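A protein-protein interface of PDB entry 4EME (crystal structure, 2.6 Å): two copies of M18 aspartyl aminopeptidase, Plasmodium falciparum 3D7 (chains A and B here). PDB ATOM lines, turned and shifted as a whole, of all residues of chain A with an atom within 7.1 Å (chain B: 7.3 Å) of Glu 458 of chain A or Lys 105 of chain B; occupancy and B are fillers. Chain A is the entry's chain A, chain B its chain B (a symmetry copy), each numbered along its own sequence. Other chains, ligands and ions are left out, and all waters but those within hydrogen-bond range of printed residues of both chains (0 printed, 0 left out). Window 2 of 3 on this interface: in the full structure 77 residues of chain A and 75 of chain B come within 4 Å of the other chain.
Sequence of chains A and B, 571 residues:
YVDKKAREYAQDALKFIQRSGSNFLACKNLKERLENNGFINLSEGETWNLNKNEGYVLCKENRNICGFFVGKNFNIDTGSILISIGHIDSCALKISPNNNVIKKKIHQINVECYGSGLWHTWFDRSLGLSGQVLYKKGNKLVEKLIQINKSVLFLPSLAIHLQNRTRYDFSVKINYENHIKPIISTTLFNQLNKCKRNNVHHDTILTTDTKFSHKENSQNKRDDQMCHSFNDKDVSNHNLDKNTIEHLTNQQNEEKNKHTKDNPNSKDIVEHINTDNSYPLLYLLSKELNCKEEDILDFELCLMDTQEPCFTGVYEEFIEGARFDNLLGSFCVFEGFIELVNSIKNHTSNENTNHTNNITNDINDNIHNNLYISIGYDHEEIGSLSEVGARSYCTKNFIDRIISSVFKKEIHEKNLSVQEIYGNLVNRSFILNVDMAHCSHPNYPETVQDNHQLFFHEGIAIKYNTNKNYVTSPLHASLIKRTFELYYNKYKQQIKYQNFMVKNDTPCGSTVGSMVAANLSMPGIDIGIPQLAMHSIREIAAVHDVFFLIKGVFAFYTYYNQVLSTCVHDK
Of the 11 printed residues of chain B, 8 touch a printed residue of chain A. Printed residues of chain B that touch a printed residue of chain A: Lys 103, Lys 104, Lys 105, Ile 106, Ser 185, Thr 186, Leu 188 and Phe 189. Hydrophobic or aromatic side chains of chain B within 4 Å of the printed part of chain A: Ile 106, Leu 188 and Phe 189. Along chain B the printed residues that touch a printed residue of chain A span positions 103 to 189. Printed residues of chain A that touch a printed residue of chain B: Glu 317, Pro 442, Gln 453, Phe 455, Phe 456, His 457, Glu 458 and His 544.
OE1 of Glu 317 of chain A lies within hydrogen-bond range of OG1 of Thr 186 of chain B (2.5 Å). The backbone carbonyl oxygen of Pro 442 of chain A lies within hydrogen-bond range of the side-chain amino group of Lys 103 of chain B. NZ of Lys 104 of chain B sits at hydrogen-bond distance from OE1 of Gln 453 of chain A (2.9 Å). OE1 of Glu 458 of chain A is in salt-bridge range of NZ of Lys 105 of chain B, at 2.8 Å.
Printed residues of chain B within 4 Å of Glu 317 of chain A: Ser 185, Thr 186 and Phe 189. Printed residues of chain B within 4 Å of Pro 442 of chain A: Lys 103 (2.8 Å), Lys 104 (3.9 Å) and Ile 106 (3.9 Å). Of chain B, only Lys 105 comes within 4 Å of Glu 458 of chain A. Ala 542 of chain A touches none of the printed residues of chain B. Of chain A, only Phe 455 (3.5 Å) and Glu 458 (2.8 Å) come within 4 Å of Lys 105 of chain B. The nearest residue of chain A that does not touch Lys 105 of chain B is Gln 498 of chain A (6.4 Å).
OE1 of Glu 317 of chain A sits at hydrogen-bond distance from NE2 of His 457 of chain A, 2.8 Å away. O of Phe 455 of chain A sits at hydrogen-bond distance from NE2 of Gln 498 of chain A (2.9 Å). OD2 of Asp 545 of chain A lies within hydrogen-bond range of N of His 457 of chain A (2.7 Å). The backbone NH (N) of Glu 458 of chain A is in hydrogen-bond range of the side-chain carboxylate (OD1) of Asp 545 of chain A. The backbone carbonyl oxygen (O) of Lys 105 of chain B sits at hydrogen-bond distance from the backbone NH (N) of Thr 187 of chain B. The backbone NH of Phe 189 of chain B lies within hydrogen-bond range of the side-chain hydroxyl of Thr 186 of chain B, 3.4 Å away.
Glu 317 of chain A touches Ser 185 of chain B. Glu 317 of chain A touches Phe 189 of chain B (OE1 to CD1, 3.3 Å). Pro 442 of chain A touches Lys 104 of chain B (CA to CG, 3.9 Å). Ile 106 of chain B touches Pro 442 of chain A. CD2 of Phe 455 of chain A touches NZ of Lys 105 of chain B (3.5 Å). Phe 456 of chain A touches Thr 186 of chain B (CB to CG2, 3.95 Å). CD2 of His 457 of chain A touches OG1 of Thr 186 of chain B (3.8 Å). CB of His 457 of chain A touches CD2 of Leu 188 of chain B, 3.8 Å away. CE1 of His 457 of chain A touches CE1 of Phe 189 of chain B (3.4 Å). Phe 189 of chain B touches His 544 of chain A.
No position is printed for both chains.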
ATOM      1  N   GLU A 317      20.248 -26.623 -30.407  1.00  0.00           N
ATOM      2  CA  GLU A 317      19.149 -26.986 -29.499  1.00  0.00           C
ATOM      3  C   GLU A 317      18.659 -28.414 -29.694  1.00  0.00           C
ATOM      4  O   GLU A 317      17.901 -28.919 -28.863  1.00  0.00           O
ATOM      5  CB  GLU A 317      17.985 -26.036 -29.699  1.00  0.00           C
ATOM      6  CG  GLU A 317      17.203 -26.331 -30.961  1.00  0.00           C
ATOM      7  CD  GLU A 317      16.074 -25.364 -31.183  1.00  0.00           C
ATOM      8  OE1 GLU A 317      15.108 -25.390 -30.391  1.00  0.00           O
ATOM      9  OE2 GLU A 317      16.200 -24.520 -32.093  1.00  0.00           O
ATOM     10  N   PRO A 442       6.048 -31.173 -38.460  1.00  0.00           N
ATOM     11  CA  PRO A 442       5.596 -29.986 -39.214  1.00  0.00           C
ATOM     12  C   PRO A 442       5.245 -30.224 -40.671  1.00  0.00           C
ATOM     13  O   PRO A 442       4.558 -29.387 -41.250  1.00  0.00           O
ATOM     14  CB  PRO A 442       6.759 -28.999 -39.068  1.00  0.00           C
ATOM     15  CG  PRO A 442       7.953 -29.850 -38.793  1.00  0.00           C
ATOM     16  CD  PRO A 442       7.430 -30.984 -37.960  1.00  0.00           C
ATOM     17  N   GLN A 453      -1.044 -32.707 -29.044  1.00  0.00           N
ATOM     18  CA  GLN A 453       0.176 -32.491 -29.824  1.00  0.00           C
ATOM     19  C   GLN A 453       1.369 -32.319 -28.896  1.00  0.00           C
ATOM     20  O   GLN A 453       1.272 -31.595 -27.897  1.00  0.00           O
ATOM     21  CB  GLN A 453       0.057 -31.241 -30.707  1.00  0.00           C
ATOM     22  CG  GLN A 453      -0.899 -31.379 -31.870  1.00  0.00           C
ATOM     23  CD  GLN A 453      -0.926 -30.115 -32.683  1.00  0.00           C
ATOM     24  OE1 GLN A 453      -0.058 -29.877 -33.524  1.00  0.00           O
ATOM     25  NE2 GLN A 453      -1.913 -29.268 -32.438  1.00  0.00           N
ATOM     26  N   LEU A 454       2.499 -32.958 -29.240  1.00  0.00           N
ATOM     27  CA  LEU A 454       3.758 -32.824 -28.504  1.00  0.00           C
ATOM     28  C   LEU A 454       4.678 -31.860 -29.248  1.00  0.00           C
ATOM     29  O   LEU A 454       4.704 -31.851 -30.476  1.00  0.00           O
ATOM     30  CB  LEU A 454       4.464 -34.167 -28.372  1.00  0.00           C
ATOM     31  CG  LEU A 454       3.776 -35.238 -27.549  1.00  0.00           C
ATOM     32  CD1 LEU A 454       4.520 -36.537 -27.685  1.00  0.00           C
ATOM     33  CD2 LEU A 454       3.602 -34.822 -26.079  1.00  0.00           C
ATOM     34  N   PHE A 455       5.426 -31.060 -28.504  1.00  0.00           N
ATOM     35  CA  PHE A 455       6.365 -30.084 -29.051  1.00  0.00           C
ATOM     36  C   PHE A 455       7.741 -30.170 -28.379  1.00  0.00           C
ATOM     37  O   PHE A 455       7.835 -30.479 -27.188  1.00  0.00           O
ATOM     38  CB  PHE A 455       5.790 -28.671 -28.927  1.00  0.00           C
ATOM     39  CG  PHE A 455       4.485 -28.470 -29.662  1.00  0.00           C
ATOM     40  CD1 PHE A 455       4.467 -28.241 -31.035  1.00  0.00           C
ATOM     41  CD2 PHE A 455       3.273 -28.508 -28.984  1.00  0.00           C
ATOM     42  CE1 PHE A 455       3.255 -28.068 -31.716  1.00  0.00           C
ATOM     43  CE2 PHE A 455       2.063 -28.333 -29.667  1.00  0.00           C
ATOM     44  CZ  PHE A 455       2.065 -28.106 -31.024  1.00  0.00           C
ATOM     45  N   PHE A 456       8.810 -29.907 -29.149  1.00  0.00           N
ATOM     46  CA  PHE A 456      10.187 -29.910 -28.657  1.00  0.00           C
ATOM     47  C   PHE A 456      10.365 -28.898 -27.516  1.00  0.00           C
ATOM     48  O   PHE A 456       9.799 -27.785 -27.569  1.00  0.00           O
ATOM     49  CB  PHE A 456      11.174 -29.613 -29.797  1.00  0.00           C
ATOM     50  CG  PHE A 456      11.429 -30.730 -30.791  1.00  0.00           C
ATOM     51  CD1 PHE A 456      11.582 -32.047 -30.365  1.00  0.00           C
ATOM     52  CD2 PHE A 456      11.593 -30.455 -32.147  1.00  0.00           C
ATOM     53  CE1 PHE A 456      11.859 -33.067 -31.276  1.00  0.00           C
ATOM     54  CE2 PHE A 456      11.864 -31.474 -33.057  1.00  0.00           C
ATOM     55  CZ  PHE A 456      12.000 -32.774 -32.612  1.00  0.00           C
ATOM     56  N   HIS A 457      11.109 -29.324 -26.452  1.00  0.00           N
ATOM     57  CA  HIS A 457      11.436 -28.551 -25.237  1.00  0.00           C
ATOM     58  C   HIS A 457      10.237 -28.340 -24.318  1.00  0.00           C
ATOM     59  O   HIS A 457      10.393 -27.746 -23.256  1.00  0.00           O
ATOM     60  CB  HIS A 457      12.086 -27.198 -25.571  1.00  0.00           C
ATOM     61  CG  HIS A 457      13.213 -27.282 -26.539  1.00  0.00           C
ATOM     62  ND1 HIS A 457      14.419 -27.845 -26.190  1.00  0.00           N
ATOM     63  CD2 HIS A 457      13.295 -26.818 -27.805  1.00  0.00           C
ATOM     64  CE1 HIS A 457      15.193 -27.721 -27.253  1.00  0.00           C
ATOM     65  NE2 HIS A 457      14.558 -27.112 -28.251  1.00  0.00           N
ATOM     66  N   GLU A 458       9.040 -28.802 -24.730  1.00  0.00           N
ATOM     67  CA  GLU A 458       7.794 -28.637 -23.985  1.00  0.00           C
ATOM     68  C   GLU A 458       7.451 -29.736 -22.969  1.00  0.00           C
ATOM     69  O   GLU A 458       6.326 -29.811 -22.463  1.00  0.00           O
ATOM     70  CB  GLU A 458       6.637 -28.232 -24.900  1.00  0.00           C
ATOM     71  CG  GLU A 458       6.697 -26.754 -25.220  1.00  0.00           C
ATOM     72  CD  GLU A 458       5.702 -26.264 -26.245  1.00  0.00           C
ATOM     73  OE1 GLU A 458       4.480 -26.403 -26.011  1.00  0.00           O
ATOM     74  OE2 GLU A 458       6.153 -25.699 -27.268  1.00  0.00           O
ATOM     75  N   GLY A 459       8.460 -30.524 -22.630  1.00  0.00           N
ATOM     76  CA  GLY A 459       8.376 -31.520 -21.580  1.00  0.00           C
ATOM     77  C   GLY A 459       8.068 -32.960 -21.905  1.00  0.00           C
ATOM     78  O   GLY A 459       7.919 -33.358 -23.062  1.00  0.00           O
ATOM     79  N   ILE A 460       8.009 -33.741 -20.819  1.00  0.00           N
ATOM     80  CA  ILE A 460       7.726 -35.161 -20.741  1.00  0.00           C
ATOM     81  C   ILE A 460       6.358 -35.440 -21.332  1.00  0.00           C
ATOM     82  O   ILE A 460       5.349 -34.860 -20.910  1.00  0.00           O
ATOM     83  CB  ILE A 460       7.821 -35.608 -19.258  1.00  0.00           C
ATOM     84  CG1 ILE A 460       9.278 -35.588 -18.767  1.00  0.00           C
ATOM     85  CG2 ILE A 460       7.159 -36.967 -19.028  1.00  0.00           C
ATOM     86  CD1 ILE A 460       9.462 -35.968 -17.324  1.00  0.00           C
ATOM     87  N   ALA A 461       6.333 -36.343 -22.314  1.00  0.00           N
ATOM     88  CA  ALA A 461       5.103 -36.782 -22.938  1.00  0.00           C
ATOM     89  C   ALA A 461       4.443 -37.819 -22.037  1.00  0.00           C
ATOM     90  O   ALA A 461       5.074 -38.811 -21.693  1.00  0.00           O
ATOM     91  CB  ALA A 461       5.404 -37.380 -24.287  1.00  0.00           C
ATOM     92  N   ILE A 495       9.256 -29.331 -13.953  1.00  0.00           N
ATOM     93  CA  ILE A 495       9.306 -30.518 -14.806  1.00  0.00           C
ATOM     94  C   ILE A 495       8.097 -30.364 -15.732  1.00  0.00           C
ATOM     95  O   ILE A 495       6.961 -30.652 -15.326  1.00  0.00           O
ATOM     96  CB  ILE A 495       9.314 -31.902 -14.058  1.00  0.00           C
ATOM     97  CG1 ILE A 495      10.571 -32.092 -13.187  1.00  0.00           C
ATOM     98  CG2 ILE A 495       9.168 -33.070 -15.063  1.00  0.00           C
ATOM     99  CD1 ILE A 495      10.405 -33.131 -12.159  1.00  0.00           C
ATOM    100  N   LYS A 496       8.339 -29.843 -16.951  1.00  0.00           N
ATOM    101  CA  LYS A 496       7.280 -29.677 -17.951  1.00  0.00           C
ATOM    102  C   LYS A 496       6.751 -31.034 -18.413  1.00  0.00           C
ATOM    103  O   LYS A 496       7.481 -32.025 -18.418  1.00  0.00           O
ATOM    104  CB  LYS A 496       7.754 -28.840 -19.150  1.00  0.00           C
ATOM    105  CG  LYS A 496       7.861 -27.362 -18.830  1.00  0.00           C
ATOM    106  CD  LYS A 496       8.365 -26.548 -19.994  1.00  0.00           C
ATOM    107  CE  LYS A 496       8.412 -25.090 -19.610  1.00  0.00           C
ATOM    108  NZ  LYS A 496       9.249 -24.301 -20.552  1.00  0.00           N
ATOM    109  N   TYR A 497       5.456 -31.086 -18.716  1.00  0.00           N
ATOM    110  CA  TYR A 497       4.808 -32.285 -19.219  1.00  0.00           C
ATOM    111  C   TYR A 497       3.756 -31.899 -20.224  1.00  0.00           C
ATOM    112  O   TYR A 497       3.241 -30.779 -20.200  1.00  0.00           O
ATOM    113  CB  TYR A 497       4.242 -33.189 -18.103  1.00  0.00           C
ATOM    114  CG  TYR A 497       3.007 -32.642 -17.421  1.00  0.00           C
ATOM    115  CD1 TYR A 497       1.733 -32.925 -17.907  1.00  0.00           C
ATOM    116  CD2 TYR A 497       3.111 -31.824 -16.301  1.00  0.00           C
ATOM    117  CE1 TYR A 497       0.595 -32.407 -17.296  1.00  0.00           C
ATOM    118  CE2 TYR A 497       1.982 -31.285 -15.693  1.00  0.00           C
ATOM    119  CZ  TYR A 497       0.725 -31.583 -16.188  1.00  0.00           C
ATOM    120  OH  TYR A 497      -0.390 -31.066 -15.565  1.00  0.00           O
ATOM    121  N   GLN A 498       3.440 -32.838 -21.113  1.00  0.00           N
ATOM    122  CA  GLN A 498       2.457 -32.676 -22.177  1.00  0.00           C
ATOM    123  C   GLN A 498       1.819 -34.019 -22.501  1.00  0.00           C
ATOM    124  O   GLN A 498       2.529 -35.009 -22.672  1.00  0.00           O
ATOM    125  CB  GLN A 498       3.083 -32.017 -23.427  1.00  0.00           C
ATOM    126  CG  GLN A 498       4.537 -32.392 -23.684  1.00  0.00           C
ATOM    127  CD  GLN A 498       5.100 -31.684 -24.880  1.00  0.00           C
ATOM    128  OE1 GLN A 498       4.447 -30.839 -25.501  1.00  0.00           O
ATOM    129  NE2 GLN A 498       6.355 -31.981 -25.198  1.00  0.00           N
ATOM    130  N   PRO A 530       9.495 -36.202 -26.787  1.00  0.00           N
ATOM    131  CA  PRO A 530       9.183 -36.079 -28.218  1.00  0.00           C
ATOM    132  C   PRO A 530      10.411 -36.099 -29.126  1.00  0.00           C
ATOM    133  O   PRO A 530      11.395 -35.394 -28.893  1.00  0.00           O
ATOM    134  CB  PRO A 530       8.417 -34.752 -28.317  1.00  0.00           C
ATOM    135  CG  PRO A 530       8.794 -33.983 -27.133  1.00  0.00           C
ATOM    136  CD  PRO A 530       9.267 -34.933 -26.062  1.00  0.00           C
ATOM    137  N   ALA A 542      15.006 -32.995 -28.760  1.00  0.00           N
ATOM    138  CA  ALA A 542      15.389 -31.684 -28.241  1.00  0.00           C
ATOM    139  C   ALA A 542      16.097 -31.793 -26.894  1.00  0.00           C
ATOM    140  O   ALA A 542      15.729 -32.626 -26.066  1.00  0.00           O
ATOM    141  CB  ALA A 542      14.172 -30.796 -28.123  1.00  0.00           C
ATOM    142  N   HIS A 544      16.329 -29.657 -24.058  1.00  0.00           N
ATOM    143  CA  HIS A 544      15.579 -29.371 -22.818  1.00  0.00           C
ATOM    144  C   HIS A 544      14.797 -30.575 -22.322  1.00  0.00           C
ATOM    145  O   HIS A 544      14.665 -30.770 -21.112  1.00  0.00           O
ATOM    146  CB  HIS A 544      14.608 -28.210 -23.014  1.00  0.00           C
ATOM    147  CG  HIS A 544      15.228 -26.849 -22.947  1.00  0.00           C
ATOM    148  ND1 HIS A 544      14.465 -25.728 -22.651  1.00  0.00           N
ATOM    149  CD2 HIS A 544      16.515 -26.464 -23.138  1.00  0.00           C
ATOM    150  CE1 HIS A 544      15.307 -24.705 -22.680  1.00  0.00           C
ATOM    151  NE2 HIS A 544      16.554 -25.102 -22.956  1.00  0.00           N
ATOM    152  N   ASP A 545      14.288 -31.391 -23.267  1.00  0.00           N
ATOM    153  CA  ASP A 545      13.486 -32.576 -22.973  1.00  0.00           C
ATOM    154  C   ASP A 545      14.289 -33.674 -22.299  1.00  0.00           C
ATOM    155  O   ASP A 545      13.736 -34.436 -21.502  1.00  0.00           O
ATOM    156  CB  ASP A 545      12.765 -33.065 -24.233  1.00  0.00           C
ATOM    157  CG  ASP A 545      11.720 -32.085 -24.756  1.00  0.00           C
ATOM    158  OD1 ASP A 545      11.032 -31.448 -23.927  1.00  0.00           O
ATOM    159  OD2 ASP A 545      11.596 -31.952 -25.988  1.00  0.00           O
ATOM    160  N   PHE A 548      14.318 -32.584 -18.609  1.00  0.00           N
ATOM    161  CA  PHE A 548      13.024 -32.852 -17.972  1.00  0.00           C
ATOM    162  C   PHE A 548      12.837 -34.311 -17.668  1.00  0.00           C
ATOM    163  O   PHE A 548      12.440 -34.643 -16.546  1.00  0.00           O
ATOM    164  CB  PHE A 548      11.833 -32.333 -18.795  1.00  0.00           C
ATOM    165  CG  PHE A 548      11.776 -30.845 -19.016  1.00  0.00           C
ATOM    166  CD1 PHE A 548      11.848 -29.965 -17.947  1.00  0.00           C
ATOM    167  CD2 PHE A 548      11.598 -30.324 -20.291  1.00  0.00           C
ATOM    168  CE1 PHE A 548      11.782 -28.589 -18.155  1.00  0.00           C
ATOM    169  CE2 PHE A 548      11.545 -28.945 -20.498  1.00  0.00           C
ATOM    170  CZ  PHE A 548      11.625 -28.090 -19.429  1.00  0.00           C
ATOM    171  N   ILE B 102       7.305 -21.279 -40.644  1.00  0.00           N
ATOM    172  CA  ILE B 102       7.087 -21.550 -39.218  1.00  0.00           C
ATOM    173  C   ILE B 102       5.838 -22.421 -39.144  1.00  0.00           C
ATOM    174  O   ILE B 102       4.749 -21.965 -39.487  1.00  0.00           O
ATOM    175  CB  ILE B 102       7.008 -20.282 -38.308  1.00  0.00           C
ATOM    176  CG1 ILE B 102       8.220 -19.336 -38.529  1.00  0.00           C
ATOM    177  CG2 ILE B 102       6.903 -20.700 -36.839  1.00  0.00           C
ATOM    178  CD1 ILE B 102       7.999 -17.907 -38.270  1.00  0.00           C
ATOM    179  N   LYS B 103       6.004 -23.688 -38.758  1.00  0.00           N
ATOM    180  CA  LYS B 103       4.904 -24.643 -38.660  1.00  0.00           C
ATOM    181  C   LYS B 103       5.119 -25.541 -37.449  1.00  0.00           C
ATOM    182  O   LYS B 103       6.230 -26.050 -37.242  1.00  0.00           O
ATOM    183  CB  LYS B 103       4.791 -25.488 -39.949  1.00  0.00           C
ATOM    184  CG  LYS B 103       4.122 -24.778 -41.136  1.00  0.00           C
ATOM    185  CD  LYS B 103       3.705 -25.751 -42.267  1.00  0.00           C
ATOM    186  CE  LYS B 103       4.767 -26.097 -43.296  1.00  0.00           C
ATOM    187  NZ  LYS B 103       5.518 -27.334 -42.943  1.00  0.00           N
ATOM    188  N   LYS B 104       4.055 -25.722 -36.635  1.00  0.00           N
ATOM    189  CA  LYS B 104       4.052 -26.552 -35.422  1.00  0.00           C
ATOM    190  C   LYS B 104       5.174 -26.134 -34.470  1.00  0.00           C
ATOM    191  O   LYS B 104       5.911 -26.985 -33.975  1.00  0.00           O
ATOM    192  CB  LYS B 104       4.122 -28.071 -35.757  1.00  0.00           C
ATOM    193  CG  LYS B 104       3.022 -28.608 -36.659  1.00  0.00           C
ATOM    194  CD  LYS B 104       1.659 -28.528 -36.007  1.00  0.00           C
ATOM    195  CE  LYS B 104       0.619 -29.278 -36.779  1.00  0.00           C
ATOM    196  NZ  LYS B 104      -0.722 -29.047 -36.197  1.00  0.00           N
ATOM    197  N   LYS B 105       5.329 -24.816 -34.259  1.00  0.00           N
ATOM    198  CA  LYS B 105       6.328 -24.192 -33.378  1.00  0.00           C
ATOM    199  C   LYS B 105       7.799 -24.420 -33.809  1.00  0.00           C
ATOM    200  O   LYS B 105       8.713 -24.163 -33.027  1.00  0.00           O
ATOM    201  CB  LYS B 105       6.088 -24.569 -31.906  1.00  0.00           C
ATOM    202  CG  LYS B 105       4.665 -24.327 -31.409  1.00  0.00           C
ATOM    203  CD  LYS B 105       4.526 -24.720 -29.959  1.00  0.00           C
ATOM    204  CE  LYS B 105       3.098 -24.761 -29.508  1.00  0.00           C
ATOM    205  NZ  LYS B 105       2.999 -25.120 -28.074  1.00  0.00           N
ATOM    206  N   ILE B 106       8.017 -24.870 -35.068  1.00  0.00           N
ATOM    207  CA  ILE B 106       9.346 -25.111 -35.638  1.00  0.00           C
ATOM    208  C   ILE B 106       9.639 -24.150 -36.818  1.00  0.00           C
ATOM    209  O   ILE B 106       8.811 -24.034 -37.726  1.00  0.00           O
ATOM    210  CB  ILE B 106       9.531 -26.613 -36.053  1.00  0.00           C
ATOM    211  CG1 ILE B 106       9.432 -27.555 -34.843  1.00  0.00           C
ATOM    212  CG2 ILE B 106      10.866 -26.836 -36.767  1.00  0.00           C
ATOM    213  CD1 ILE B 106       9.254 -28.992 -35.187  1.00  0.00           C
ATOM    214  N   HIS B 107      10.830 -23.495 -36.808  1.00  0.00           N
ATOM    215  CA  HIS B 107      11.306 -22.650 -37.908  1.00  0.00           C
ATOM    216  C   HIS B 107      11.882 -23.578 -38.962  1.00  0.00           C
ATOM    217  O   HIS B 107      12.759 -24.408 -38.673  1.00  0.00           O
ATOM    218  CB  HIS B 107      12.398 -21.672 -37.456  1.00  0.00           C
ATOM    219  CG  HIS B 107      11.880 -20.460 -36.742  1.00  0.00           C
ATOM    220  ND1 HIS B 107      11.746 -19.241 -37.386  1.00  0.00           N
ATOM    221  CD2 HIS B 107      11.514 -20.315 -35.448  1.00  0.00           C
ATOM    222  CE1 HIS B 107      11.308 -18.405 -36.464  1.00  0.00           C
ATOM    223  NE2 HIS B 107      11.160 -19.007 -35.284  1.00  0.00           N
ATOM    224  N   SER B 185      15.424 -24.522 -36.430  1.00  0.00           N
ATOM    225  CA  SER B 185      15.250 -24.214 -35.014  1.00  0.00           C
ATOM    226  C   SER B 185      13.789 -24.328 -34.627  1.00  0.00           C
ATOM    227  O   SER B 185      12.926 -24.527 -35.469  1.00  0.00           O
ATOM    228  CB  SER B 185      15.711 -22.781 -34.729  1.00  0.00           C
ATOM    229  OG  SER B 185      14.656 -21.840 -34.882  1.00  0.00           O
ATOM    230  N   THR B 186      13.513 -24.115 -33.354  1.00  0.00           N
ATOM    231  CA  THR B 186      12.164 -23.997 -32.799  1.00  0.00           C
ATOM    232  C   THR B 186      11.930 -22.492 -32.578  1.00  0.00           C
ATOM    233  O   THR B 186      12.883 -21.695 -32.595  1.00  0.00           O
ATOM    234  CB  THR B 186      12.036 -24.751 -31.462  1.00  0.00           C
ATOM    235  OG1 THR B 186      12.964 -24.202 -30.523  1.00  0.00           O
ATOM    236  CG2 THR B 186      12.209 -26.256 -31.605  1.00  0.00           C
ATOM    237  N   THR B 187      10.685 -22.110 -32.350  1.00  0.00           N
ATOM    238  CA  THR B 187      10.336 -20.724 -32.058  1.00  0.00           C
ATOM    239  C   THR B 187      10.882 -20.308 -30.697  1.00  0.00           C
ATOM    240  O   THR B 187      11.279 -19.152 -30.544  1.00  0.00           O
ATOM    241  CB  THR B 187       8.829 -20.492 -32.189  1.00  0.00           C
ATOM    242  OG1 THR B 187       8.127 -21.541 -31.518  1.00  0.00           O
ATOM    243  CG2 THR B 187       8.387 -20.420 -33.627  1.00  0.00           C
ATOM    244  N   LEU B 188      10.944 -21.254 -29.722  1.00  0.00           N
ATOM    245  CA  LEU B 188      11.460 -20.995 -28.374  1.00  0.00           C
ATOM    246  C   LEU B 188      12.890 -20.462 -28.416  1.00  0.00           C
ATOM    247  O   LEU B 188      13.130 -19.342 -27.953  1.00  0.00           O
ATOM    248  CB  LEU B 188      11.376 -22.248 -27.476  1.00  0.00           C
ATOM    249  CG  LEU B 188      11.943 -22.090 -26.038  1.00  0.00           C
ATOM    250  CD1 LEU B 188      11.106 -21.134 -25.194  1.00  0.00           C
ATOM    251  CD2 LEU B 188      12.039 -23.416 -25.331  1.00  0.00           C
ATOM    252  N   PHE B 189      13.823 -21.252 -28.999  1.00  0.00           N
ATOM    253  CA  PHE B 189      15.240 -20.903 -29.096  1.00  0.00           C
ATOM    254  C   PHE B 189      15.536 -19.662 -29.942  1.00  0.00           C
ATOM    255  O   PHE B 189      16.449 -18.906 -29.595  1.00  0.00           O
ATOM    256  CB  PHE B 189      16.098 -22.118 -29.470  1.00  0.00           C
ATOM    257  CG  PHE B 189      16.494 -22.979 -28.291  1.00  0.00           C
ATOM    258  CD1 PHE B 189      15.540 -23.721 -27.594  1.00  0.00           C
ATOM    259  CD2 PHE B 189      17.821 -23.070 -27.890  1.00  0.00           C
ATOM    260  CE1 PHE B 189      15.906 -24.518 -26.508  1.00  0.00           C
ATOM    261  CE2 PHE B 189      18.190 -23.888 -26.819  1.00  0.00           C
ATOM    262  CZ  PHE B 189      17.231 -24.616 -26.145  1.00  0.00           C
